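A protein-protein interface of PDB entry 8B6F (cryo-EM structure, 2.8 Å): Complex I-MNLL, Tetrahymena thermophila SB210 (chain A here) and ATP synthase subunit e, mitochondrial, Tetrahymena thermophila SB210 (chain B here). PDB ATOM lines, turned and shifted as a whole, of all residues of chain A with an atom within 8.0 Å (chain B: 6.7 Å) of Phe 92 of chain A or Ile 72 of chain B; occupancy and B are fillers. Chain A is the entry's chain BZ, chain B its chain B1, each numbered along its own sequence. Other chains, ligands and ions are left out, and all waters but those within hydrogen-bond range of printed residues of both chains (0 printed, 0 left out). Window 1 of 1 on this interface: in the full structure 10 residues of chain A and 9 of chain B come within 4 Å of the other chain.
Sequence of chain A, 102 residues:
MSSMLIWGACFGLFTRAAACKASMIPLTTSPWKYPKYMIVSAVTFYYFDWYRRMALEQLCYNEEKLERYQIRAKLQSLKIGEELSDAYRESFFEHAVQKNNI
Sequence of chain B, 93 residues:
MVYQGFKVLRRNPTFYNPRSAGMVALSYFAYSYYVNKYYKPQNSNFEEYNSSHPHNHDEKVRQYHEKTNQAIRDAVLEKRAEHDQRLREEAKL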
ATOM      1  N   LEU A  75      -2.633   5.886  33.477  1.00  0.00           N
ATOM      2  CA  LEU A  75      -1.488   5.224  32.858  1.00  0.00           C
ATOM      3  C   LEU A  75      -1.043   4.015  33.670  1.00  0.00           C
ATOM      4  O   LEU A  75      -0.678   2.980  33.104  1.00  0.00           O
ATOM      5  CB  LEU A  75      -0.336   6.214  32.693  1.00  0.00           C
ATOM      6  CG  LEU A  75      -0.583   7.386  31.740  1.00  0.00           C
ATOM      7  CD1 LEU A  75       0.605   8.327  31.735  1.00  0.00           C
ATOM      8  CD2 LEU A  75      -0.871   6.900  30.332  1.00  0.00           C
ATOM      9  N   GLN A  76      -1.059   4.130  34.998  1.00  0.00           N
ATOM     10  CA  GLN A  76      -0.677   3.008  35.845  1.00  0.00           C
ATOM     11  C   GLN A  76      -1.747   1.926  35.892  1.00  0.00           C
ATOM     12  O   GLN A  76      -1.431   0.776  36.214  1.00  0.00           O
ATOM     13  CB  GLN A  76      -0.376   3.501  37.258  1.00  0.00           C
ATOM     14  CG  GLN A  76       0.780   4.476  37.326  1.00  0.00           C
ATOM     15  CD  GLN A  76       1.034   4.971  38.729  1.00  0.00           C
ATOM     16  OE1 GLN A  76       1.798   4.370  39.481  1.00  0.00           O
ATOM     17  NE2 GLN A  76       0.392   6.073  39.094  1.00  0.00           N
ATOM     18  N   LEU A  78      -3.258   0.831  33.266  1.00  0.00           N
ATOM     19  CA  LEU A  78      -3.222   0.101  32.008  1.00  0.00           C
ATOM     20  C   LEU A  78      -2.870  -1.360  32.246  1.00  0.00           C
ATOM     21  O   LEU A  78      -1.977  -1.682  33.034  1.00  0.00           O
ATOM     22  CB  LEU A  78      -2.205   0.736  31.059  1.00  0.00           C
ATOM     23  CG  LEU A  78      -2.464   2.191  30.670  1.00  0.00           C
ATOM     24  CD1 LEU A  78      -1.302   2.736  29.861  1.00  0.00           C
ATOM     25  CD2 LEU A  78      -3.761   2.320  29.894  1.00  0.00           C
ATOM     26  N   LYS A  79      -3.581  -2.247  31.558  1.00  0.00           N
ATOM     27  CA  LYS A  79      -3.308  -3.668  31.672  1.00  0.00           C
ATOM     28  C   LYS A  79      -1.937  -3.989  31.090  1.00  0.00           C
ATOM     29  O   LYS A  79      -1.397  -3.260  30.255  1.00  0.00           O
ATOM     30  CB  LYS A  79      -4.390  -4.484  30.963  1.00  0.00           C
ATOM     31  CG  LYS A  79      -5.647  -4.712  31.794  1.00  0.00           C
ATOM     32  CD  LYS A  79      -6.355  -3.410  32.130  1.00  0.00           C
ATOM     33  CE  LYS A  79      -7.626  -3.670  32.925  1.00  0.00           C
ATOM     34  NZ  LYS A  79      -8.336  -2.407  33.271  1.00  0.00           N
ATOM     35  N   ILE A  80      -1.367  -5.103  31.554  1.00  0.00           N
ATOM     36  CA  ILE A  80      -0.040  -5.504  31.107  1.00  0.00           C
ATOM     37  C   ILE A  80      -0.028  -5.608  29.590  1.00  0.00           C
ATOM     38  O   ILE A  80      -0.899  -6.243  28.984  1.00  0.00           O
ATOM     39  CB  ILE A  80       0.367  -6.827  31.774  1.00  0.00           C
ATOM     40  CG1 ILE A  80       1.815  -7.190  31.433  1.00  0.00           C
ATOM     41  CG2 ILE A  80      -0.570  -7.956  31.360  1.00  0.00           C
ATOM     42  CD1 ILE A  80       2.839  -6.236  31.997  1.00  0.00           C
ATOM     43  N   GLY A  81       0.959  -4.965  28.966  1.00  0.00           N
ATOM     44  CA  GLY A  81       1.117  -4.984  27.533  1.00  0.00           C
ATOM     45  C   GLY A  81       0.562  -3.768  26.823  1.00  0.00           C
ATOM     46  O   GLY A  81       0.933  -3.522  25.670  1.00  0.00           O
ATOM     47  N   GLU A  82      -0.313  -3.006  27.474  1.00  0.00           N
ATOM     48  CA  GLU A  82      -0.916  -1.833  26.858  1.00  0.00           C
ATOM     49  C   GLU A  82      -0.080  -0.573  27.012  1.00  0.00           C
ATOM     50  O   GLU A  82      -0.348   0.414  26.320  1.00  0.00           O
ATOM     51  CB  GLU A  82      -2.293  -1.578  27.474  1.00  0.00           C
ATOM     52  CG  GLU A  82      -3.269  -2.717  27.287  1.00  0.00           C
ATOM     53  CD  GLU A  82      -4.650  -2.382  27.805  1.00  0.00           C
ATOM     54  OE1 GLU A  82      -4.878  -1.213  28.176  1.00  0.00           O
ATOM     55  OE2 GLU A  82      -5.509  -3.285  27.836  1.00  0.00           O
ATOM     56  N   GLU A  83       0.924  -0.577  27.889  1.00  0.00           N
ATOM     57  CA  GLU A  83       1.709   0.632  28.109  1.00  0.00           C
ATOM     58  C   GLU A  83       2.650   0.930  26.950  1.00  0.00           C
ATOM     59  O   GLU A  83       3.089   2.075  26.809  1.00  0.00           O
ATOM     60  CB  GLU A  83       2.504   0.532  29.415  1.00  0.00           C
ATOM     61  CG  GLU A  83       3.175  -0.807  29.662  1.00  0.00           C
ATOM     62  CD  GLU A  83       2.288  -1.780  30.420  1.00  0.00           C
ATOM     63  OE1 GLU A  83       1.107  -1.453  30.653  1.00  0.00           O
ATOM     64  OE2 GLU A  83       2.770  -2.873  30.783  1.00  0.00           O
ATOM     65  N   LEU A  84       2.965  -0.065  26.121  1.00  0.00           N
ATOM     66  CA  LEU A  84       3.777   0.137  24.928  1.00  0.00           C
ATOM     67  C   LEU A  84       2.958   0.036  23.649  1.00  0.00           C
ATOM     68  O   LEU A  84       3.531   0.027  22.555  1.00  0.00           O
ATOM     69  CB  LEU A  84       4.932  -0.868  24.894  1.00  0.00           C
ATOM     70  CG  LEU A  84       6.055  -0.665  25.916  1.00  0.00           C
ATOM     71  CD1 LEU A  84       7.095  -1.763  25.779  1.00  0.00           C
ATOM     72  CD2 LEU A  84       6.709   0.701  25.773  1.00  0.00           C
ATOM     73  N   SER A  85       1.636  -0.038  23.761  1.00  0.00           N
ATOM     74  CA  SER A  85       0.781  -0.087  22.587  1.00  0.00           C
ATOM     75  C   SER A  85       0.748   1.278  21.902  1.00  0.00           C
ATOM     76  O   SER A  85       1.103   2.306  22.482  1.00  0.00           O
ATOM     77  CB  SER A  85      -0.632  -0.525  22.970  1.00  0.00           C
ATOM     78  OG  SER A  85      -1.205   0.357  23.919  1.00  0.00           O
ATOM     79  N   ALA A  87      -1.666   3.111  21.240  1.00  0.00           N
ATOM     80  CA  ALA A  87      -2.634   4.039  21.808  1.00  0.00           C
ATOM     81  C   ALA A  87      -2.160   4.693  23.096  1.00  0.00           C
ATOM     82  O   ALA A  87      -2.747   5.697  23.513  1.00  0.00           O
ATOM     83  CB  ALA A  87      -3.960   3.321  22.074  1.00  0.00           C
ATOM     84  N   TYR A  88      -1.122   4.153  23.738  1.00  0.00           N
ATOM     85  CA  TYR A  88      -0.629   4.695  24.996  1.00  0.00           C
ATOM     86  C   TYR A  88       0.884   4.844  25.047  1.00  0.00           C
ATOM     87  O   TYR A  88       1.393   5.394  26.030  1.00  0.00           O
ATOM     88  CB  TYR A  88      -1.068   3.805  26.170  1.00  0.00           C
ATOM     89  CG  TYR A  88      -2.565   3.677  26.321  1.00  0.00           C
ATOM     90  CD1 TYR A  88      -3.328   4.729  26.806  1.00  0.00           C
ATOM     91  CD2 TYR A  88      -3.215   2.493  25.995  1.00  0.00           C
ATOM     92  CE1 TYR A  88      -4.695   4.612  26.951  1.00  0.00           C
ATOM     93  CE2 TYR A  88      -4.582   2.366  26.137  1.00  0.00           C
ATOM     94  CZ  TYR A  88      -5.316   3.429  26.616  1.00  0.00           C
ATOM     95  OH  TYR A  88      -6.677   3.311  26.761  1.00  0.00           O
ATOM     96  N   ARG A  89       1.615   4.386  24.031  1.00  0.00           N
ATOM     97  CA  ARG A  89       3.074   4.389  24.100  1.00  0.00           C
ATOM     98  C   ARG A  89       3.619   5.808  24.213  1.00  0.00           C
ATOM     99  O   ARG A  89       4.494   6.086  25.041  1.00  0.00           O
ATOM    100  CB  ARG A  89       3.653   3.684  22.875  1.00  0.00           C
ATOM    101  CG  ARG A  89       5.162   3.786  22.762  1.00  0.00           C
ATOM    102  CD  ARG A  89       5.702   2.833  21.712  1.00  0.00           C
ATOM    103  NE  ARG A  89       4.921   2.889  20.482  1.00  0.00           N
ATOM    104  CZ  ARG A  89       5.093   3.784  19.519  1.00  0.00           C
ATOM    105  NH1 ARG A  89       6.014   4.728  19.609  1.00  0.00           N
ATOM    106  NH2 ARG A  89       4.318   3.732  18.440  1.00  0.00           N
ATOM    107  N   GLU A  90       3.116   6.721  23.383  1.00  0.00           N
ATOM    108  CA  GLU A  90       3.633   8.085  23.391  1.00  0.00           C
ATOM    109  C   GLU A  90       3.338   8.774  24.715  1.00  0.00           C
ATOM    110  O   GLU A  90       4.201   9.465  25.269  1.00  0.00           O
ATOM    111  CB  GLU A  90       3.039   8.879  22.230  1.00  0.00           C
ATOM    112  CG  GLU A  90       3.602  10.282  22.104  1.00  0.00           C
ATOM    113  CD  GLU A  90       3.072  11.009  20.887  1.00  0.00           C
ATOM    114  OE1 GLU A  90       2.379  10.369  20.069  1.00  0.00           O
ATOM    115  OE2 GLU A  90       3.344  12.220  20.751  1.00  0.00           O
ATOM    116  N   SER A  91       2.123   8.605  25.233  1.00  0.00           N
ATOM    117  CA  SER A  91       1.773   9.210  26.512  1.00  0.00           C
ATOM    118  C   SER A  91       2.589   8.618  27.652  1.00  0.00           C
ATOM    119  O   SER A  91       3.027   9.343  28.551  1.00  0.00           O
ATOM    120  CB  SER A  91       0.286   9.004  26.777  1.00  0.00           C
ATOM    121  OG  SER A  91      -0.103   9.612  27.987  1.00  0.00           O
ATOM    122  N   PHE A  92       2.803   7.304  27.635  1.00  0.00           N
ATOM    123  CA  PHE A  92       3.610   6.675  28.673  1.00  0.00           C
ATOM    124  C   PHE A  92       5.037   7.204  28.658  1.00  0.00           C
ATOM    125  O   PHE A  92       5.616   7.486  29.712  1.00  0.00           O
ATOM    126  CB  PHE A  92       3.594   5.158  28.502  1.00  0.00           C
ATOM    127  CG  PHE A  92       4.393   4.428  29.536  1.00  0.00           C
ATOM    128  CD1 PHE A  92       3.818   4.051  30.737  1.00  0.00           C
ATOM    129  CD2 PHE A  92       5.722   4.112  29.304  1.00  0.00           C
ATOM    130  CE1 PHE A  92       4.554   3.379  31.692  1.00  0.00           C
ATOM    131  CE2 PHE A  92       6.464   3.440  30.253  1.00  0.00           C
ATOM    132  CZ  PHE A  92       5.878   3.071  31.449  1.00  0.00           C
ATOM    133  N   PHE A  93       5.620   7.352  27.468  1.00  0.00           N
ATOM    134  CA  PHE A  93       6.963   7.913  27.371  1.00  0.00           C
ATOM    135  C   PHE A  93       6.986   9.371  27.805  1.00  0.00           C
ATOM    136  O   PHE A  93       7.972   9.830  28.393  1.00  0.00           O
ATOM    137  CB  PHE A  93       7.492   7.771  25.943  1.00  0.00           C
ATOM    138  CG  PHE A  93       7.885   6.366  25.571  1.00  0.00           C
ATOM    139  CD1 PHE A  93       8.441   5.506  26.507  1.00  0.00           C
ATOM    140  CD2 PHE A  93       7.702   5.909  24.278  1.00  0.00           C
ATOM    141  CE1 PHE A  93       8.802   4.221  26.159  1.00  0.00           C
ATOM    142  CE2 PHE A  93       8.062   4.624  23.925  1.00  0.00           C
ATOM    143  CZ  PHE A  93       8.612   3.780  24.868  1.00  0.00           C
ATOM    144  N   GLU A  94       5.922  10.122  27.520  1.00  0.00           N
ATOM    145  CA  GLU A  94       5.869  11.504  27.982  1.00  0.00           C
ATOM    146  C   GLU A  94       5.892  11.577  29.503  1.00  0.00           C
ATOM    147  O   GLU A  94       6.586  12.420  30.081  1.00  0.00           O
ATOM    148  CB  GLU A  94       4.619  12.191  27.431  1.00  0.00           C
ATOM    149  CG  GLU A  94       4.427  13.615  27.934  1.00  0.00           C
ATOM    150  CD  GLU A  94       3.205  14.284  27.337  1.00  0.00           C
ATOM    151  OE1 GLU A  94       2.650  13.748  26.355  1.00  0.00           O
ATOM    152  OE2 GLU A  94       2.796  15.344  27.855  1.00  0.00           O
ATOM    153  N   HIS A  95       5.137  10.706  30.172  1.00  0.00           N
ATOM    154  CA  HIS A  95       5.075  10.737  31.627  1.00  0.00           C
ATOM    155  C   HIS A  95       6.257  10.046  32.290  1.00  0.00           C
ATOM    156  O   HIS A  95       6.484  10.256  33.486  1.00  0.00           O
ATOM    157  CB  HIS A  95       3.774  10.096  32.111  1.00  0.00           C
ATOM    158  CG  HIS A  95       2.600  11.023  32.072  1.00  0.00           C
ATOM    159  ND1 HIS A  95       1.891  11.279  30.919  1.00  0.00           N
ATOM    160  CD2 HIS A  95       2.018  11.765  33.043  1.00  0.00           C
ATOM    161  CE1 HIS A  95       0.919  12.134  31.182  1.00  0.00           C
ATOM    162  NE2 HIS A  95       0.975  12.445  32.464  1.00  0.00           N
ATOM    163  N   ALA A  96       7.011   9.231  31.554  1.00  0.00           N
ATOM    164  CA  ALA A  96       8.140   8.510  32.124  1.00  0.00           C
ATOM    165  C   ALA A  96       9.489   9.125  31.781  1.00  0.00           C
ATOM    166  O   ALA A  96      10.486   8.772  32.417  1.00  0.00           O
ATOM    167  CB  ALA A  96       8.124   7.050  31.656  1.00  0.00           C
ATOM    168  N   VAL A  97       9.547  10.024  30.800  1.00  0.00           N
ATOM    169  CA  VAL A  97      10.815  10.594  30.359  1.00  0.00           C
ATOM    170  C   VAL A  97      10.775  12.107  30.512  1.00  0.00           C
ATOM    171  O   VAL A  97      11.603  12.694  31.217  1.00  0.00           O
ATOM    172  CB  VAL A  97      11.125  10.195  28.905  1.00  0.00           C
ATOM    173  CG1 VAL A  97      12.451  10.790  28.457  1.00  0.00           C
ATOM    174  CG2 VAL A  97      11.147   8.685  28.765  1.00  0.00           C
ATOM    175  N   GLN A  98       9.813  12.750  29.847  1.00  0.00           N
ATOM    176  CA  GLN A  98       9.740  14.206  29.885  1.00  0.00           C
ATOM    177  C   GLN A  98       9.486  14.711  31.299  1.00  0.00           C
ATOM    178  O   GLN A  98      10.083  15.704  31.729  1.00  0.00           O
ATOM    179  CB  GLN A  98       8.649  14.701  28.934  1.00  0.00           C
ATOM    180  CG  GLN A  98       8.803  14.202  27.506  1.00  0.00           C
ATOM    181  CD  GLN A  98      10.134  14.586  26.892  1.00  0.00           C
ATOM    182  OE1 GLN A  98      10.757  15.566  27.300  1.00  0.00           O
ATOM    183  NE2 GLN A  98      10.580  13.810  25.912  1.00  0.00           N
ATOM    184  N   LYS A  99       8.607  14.040  32.039  1.00  0.00           N
ATOM    185  CA  LYS A  99       8.268  14.440  33.398  1.00  0.00           C
ATOM    186  C   LYS A  99       9.223  13.868  34.438  1.00  0.00           C
ATOM    187  O   LYS A  99       9.027  14.106  35.634  1.00  0.00           O
ATOM    188  CB  LYS A  99       6.834  14.024  33.732  1.00  0.00           C
ATOM    189  CG  LYS A  99       5.786  14.744  32.899  1.00  0.00           C
ATOM    190  CD  LYS A  99       4.380  14.417  33.371  1.00  0.00           C
ATOM    191  CE  LYS A  99       3.335  15.038  32.461  1.00  0.00           C
ATOM    192  NZ  LYS A  99       3.462  16.519  32.381  1.00  0.00           N
ATOM    193  N   HIS B  65       4.335 -11.468  31.598  1.00  0.00           N
ATOM    194  CA  HIS B  65       4.532 -10.333  32.493  1.00  0.00           C
ATOM    195  C   HIS B  65       6.013 -10.009  32.630  1.00  0.00           C
ATOM    196  O   HIS B  65       6.415  -8.843  32.570  1.00  0.00           O
ATOM    197  CB  HIS B  65       3.925 -10.632  33.865  1.00  0.00           C
ATOM    198  CG  HIS B  65       2.451 -10.386  33.945  1.00  0.00           C
ATOM    199  ND1 HIS B  65       1.904  -9.413  34.754  1.00  0.00           N
ATOM    200  CD2 HIS B  65       1.409 -10.990  33.329  1.00  0.00           C
ATOM    201  CE1 HIS B  65       0.590  -9.427  34.630  1.00  0.00           C
ATOM    202  NE2 HIS B  65       0.263 -10.375  33.771  1.00  0.00           N
ATOM    203  N   LYS B  67       8.621 -10.686  30.585  1.00  0.00           N
ATOM    204  CA  LYS B  67       9.215 -10.124  29.376  1.00  0.00           C
ATOM    205  C   LYS B  67       8.698  -8.717  29.109  1.00  0.00           C
ATOM    206  O   LYS B  67       9.459  -7.845  28.676  1.00  0.00           O
ATOM    207  CB  LYS B  67       8.943 -11.033  28.178  1.00  0.00           C
ATOM    208  CG  LYS B  67       7.477 -11.172  27.824  1.00  0.00           C
ATOM    209  CD  LYS B  67       7.263 -12.148  26.674  1.00  0.00           C
ATOM    210  CE  LYS B  67       7.855 -11.635  25.368  1.00  0.00           C
ATOM    211  NZ  LYS B  67       7.302 -10.311  24.973  1.00  0.00           N
ATOM    212  N   THR B  68       7.408  -8.477  29.353  1.00  0.00           N
ATOM    213  CA  THR B  68       6.856  -7.146  29.128  1.00  0.00           C
ATOM    214  C   THR B  68       7.483  -6.123  30.065  1.00  0.00           C
ATOM    215  O   THR B  68       7.824  -5.012  29.644  1.00  0.00           O
ATOM    216  CB  THR B  68       5.338  -7.173  29.306  1.00  0.00           C
ATOM    217  OG1 THR B  68       4.762  -8.099  28.378  1.00  0.00           O
ATOM    218  CG2 THR B  68       4.742  -5.792  29.072  1.00  0.00           C
ATOM    219  N   ASN B  69       7.648  -6.478  31.341  1.00  0.00           N
ATOM    220  CA  ASN B  69       8.291  -5.560  32.276  1.00  0.00           C
ATOM    221  C   ASN B  69       9.734  -5.296  31.871  1.00  0.00           C
ATOM    222  O   ASN B  69      10.210  -4.159  31.952  1.00  0.00           O
ATOM    223  CB  ASN B  69       8.225  -6.124  33.694  1.00  0.00           C
ATOM    224  CG  ASN B  69       6.809  -6.220  34.216  1.00  0.00           C
ATOM    225  OD1 ASN B  69       5.974  -5.360  33.941  1.00  0.00           O
ATOM    226  ND2 ASN B  69       6.529  -7.274  34.970  1.00  0.00           N
ATOM    227  N   GLN B  70      10.449  -6.336  31.441  1.00  0.00           N
ATOM    228  CA  GLN B  70      11.822  -6.143  30.991  1.00  0.00           C
ATOM    229  C   GLN B  70      11.873  -5.195  29.801  1.00  0.00           C
ATOM    230  O   GLN B  70      12.715  -4.291  29.751  1.00  0.00           O
ATOM    231  CB  GLN B  70      12.451  -7.491  30.634  1.00  0.00           C
ATOM    232  CG  GLN B  70      13.913  -7.406  30.223  1.00  0.00           C
ATOM    233  CD  GLN B  70      14.805  -6.909  31.341  1.00  0.00           C
ATOM    234  OE1 GLN B  70      15.175  -7.666  32.237  1.00  0.00           O
ATOM    235  NE2 GLN B  70      15.157  -5.629  31.294  1.00  0.00           N
ATOM    236  N   ALA B  71      10.973  -5.383  28.835  1.00  0.00           N
ATOM    237  CA  ALA B  71      10.950  -4.512  27.667  1.00  0.00           C
ATOM    238  C   ALA B  71      10.632  -3.076  28.060  1.00  0.00           C
ATOM    239  O   ALA B  71      11.241  -2.134  27.543  1.00  0.00           O
ATOM    240  CB  ALA B  71       9.932  -5.027  26.650  1.00  0.00           C
ATOM    241  N   ILE B  72       9.673  -2.888  28.968  1.00  0.00           N
ATOM    242  CA  ILE B  72       9.327  -1.541  29.414  1.00  0.00           C
ATOM    243  C   ILE B  72      10.531  -0.873  30.062  1.00  0.00           C
ATOM    244  O   ILE B  72      10.852   0.284  29.774  1.00  0.00           O
ATOM    245  CB  ILE B  72       8.126  -1.589  30.375  1.00  0.00           C
ATOM    246  CG1 ILE B  72       6.875  -2.064  29.639  1.00  0.00           C
ATOM    247  CG2 ILE B  72       7.874  -0.223  30.996  1.00  0.00           C
ATOM    248  CD1 ILE B  72       5.810  -2.600  30.558  1.00  0.00           C
ATOM    249  N   ARG B  73      11.217  -1.595  30.952  1.00  0.00           N
ATOM    250  CA  ARG B  73      12.373  -1.013  31.625  1.00  0.00           C
ATOM    251  C   ARG B  73      13.465  -0.654  30.629  1.00  0.00           C
ATOM    252  O   ARG B  73      14.054   0.430  30.707  1.00  0.00           O
ATOM    253  CB  ARG B  73      12.907  -1.981  32.681  1.00  0.00           C
ATOM    254  CG  ARG B  73      12.000  -2.137  33.890  1.00  0.00           C
ATOM    255  CD  ARG B  73      12.719  -2.840  35.030  1.00  0.00           C
ATOM    256  NE  ARG B  73      13.129  -4.193  34.674  1.00  0.00           N
ATOM    257  CZ  ARG B  73      12.395  -5.281  34.866  1.00  0.00           C
ATOM    258  NH1 ARG B  73      11.191  -5.217  35.411  1.00  0.00           N
ATOM    259  NH2 ARG B  73      12.880  -6.464  34.502  1.00  0.00           N
ATOM    260  N   ASP B  74      13.752  -1.549  29.683  1.00  0.00           N
ATOM    261  CA  ASP B  74      14.790  -1.267  28.697  1.00  0.00           C
ATOM    262  C   ASP B  74      14.439  -0.041  27.866  1.00  0.00           C
ATOM    263  O   ASP B  74      15.274   0.845  27.659  1.00  0.00           O
ATOM    264  CB  ASP B  74      15.000  -2.481  27.791  1.00  0.00           C
ATOM    265  CG  ASP B  74      15.618  -3.653  28.522  1.00  0.00           C
ATOM    266  OD1 ASP B  74      15.965  -3.498  29.711  1.00  0.00           O
ATOM    267  OD2 ASP B  74      15.760  -4.731  27.907  1.00  0.00           O
ATOM    268  N   ALA B  75      13.200   0.026  27.376  1.00  0.00           N
ATOM    269  CA  ALA B  75      12.808   1.153  26.539  1.00  0.00           C
ATOM    270  C   ALA B  75      12.880   2.467  27.303  1.00  0.00           C
ATOM    271  O   ALA B  75      13.364   3.474  26.773  1.00  0.00           O
ATOM    272  CB  ALA B  75      11.396   0.932  25.996  1.00  0.00           C
ATOM    273  N   VAL B  76      12.404   2.482  28.548  1.00  0.00           N
ATOM    274  CA  VAL B  76      12.403   3.724  29.314  1.00  0.00           C
ATOM    275  C   VAL B  76      13.826   4.145  29.659  1.00  0.00           C
ATOM    276  O   VAL B  76      14.155   5.335  29.639  1.00  0.00           O
ATOM    277  CB  VAL B  76      11.531   3.591  30.574  1.00  0.00           C
ATOM    278  CG1 VAL B  76      11.652   4.852  31.415  1.00  0.00           C
ATOM    279  CG2 VAL B  76      10.083   3.332  30.198  1.00  0.00           C
ATOM    280  N   LEU B  77      14.688   3.183  29.992  1.00  0.00           N
ATOM    281  CA  LEU B  77      16.081   3.520  30.259  1.00  0.00           C
ATOM    282  C   LEU B  77      16.739   4.127  29.028  1.00  0.00           C
ATOM    283  O   LEU B  77      17.452   5.131  29.126  1.00  0.00           O
ATOM    284  CB  LEU B  77      16.848   2.279  30.718  1.00  0.00           C
ATOM    285  CG  LEU B  77      17.032   2.102  32.228  1.00  0.00           C
ATOM    286  CD1 LEU B  77      18.009   3.134  32.770  1.00  0.00           C
ATOM    287  CD2 LEU B  77      15.701   2.186  32.962  1.00  0.00           C
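The side-chain amide nitrogen (ND2) of Asn 69 of chain B lies within hydrogen-bond range of the backbone carbonyl oxygen (O) of His 65 of chain B (2.9 Å). N of Gly 81 of chain A lies within hydrogen-bond range of OE2 of Glu 83 of chain A (3.3 Å).
Of the 12 printed residues of chain B, 5 touch a printed residue of chain A. Along chain B the printed residues that touch a printed residue of chain A span positions 65 to 76. Of the 23 printed residues of chain A, 5 touch a printed residue of chain B. Printed residues of chain A that touch a printed residue of chain B: Ile 80, Gly 81, Glu 83, Leu 84 and Phe 92. Hydrophobic or aromatic side chains of chain A within 4 Å of the printed part of chain B: Ile 80, Leu 84 and Phe 92. Among the printed residues, no Asp or Glu carboxylate lies within 4 Å of a Lys or Arg side-chain nitrogen of the other chain.
Of the printed residues of chain B, Gly 81 of chain A touches Thr 68. Printed residues of chain B within 4 Å of Glu 83 of chain A: Thr 68 and Ile 72. Phe 92 of chain A touches just these residues of chain B: Ile 72 and Val 76. Glu 94 of chain A touches none of the printed residues of chain B. Printed residues of chain A within 4 Å of His 65 of chain B: Ile 80 (3.5 Å). Of the printed residues of chain A, Thr 68 of chain B touches Ile 80 (3.5 Å), Gly 81 (3.9 Å) and Glu 83 (3.9 Å). Printed residues of chain A within 4 Å of Asn 69 of chain B: Ile 80. Ala 71 of chain B touches none of the printed residues of chain A. Ile 72 of chain B touches three residues of chain A. Arg 73 of chain B touches none of the printed residues of chain A.
Among the printed residues, pairs that only touch across the chains: Glu 83 of chain A with Ile 72 of chain B (3.1 Å), Ile 80 of chain A with His 65 of chain B (3.5 Å), Ile 80 of chain A with Thr 68 of chain B (3.5 Å), Phe 92 of chain A with Val 76 of chain B (3.6 Å), Ile 80 of chain A with Asn 69 of chain B (3.8 Å), Gly 81 of chain A with Thr 68 of chain B (3.9 Å), Leu 84 of chain A with Ile 72 of chain B (3.9 Å), Phe 92 of chain A with Ile 72 of chain B (3.9 Å) and Glu 83 of chain A with Thr 68 of chain B (3.9 Å).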
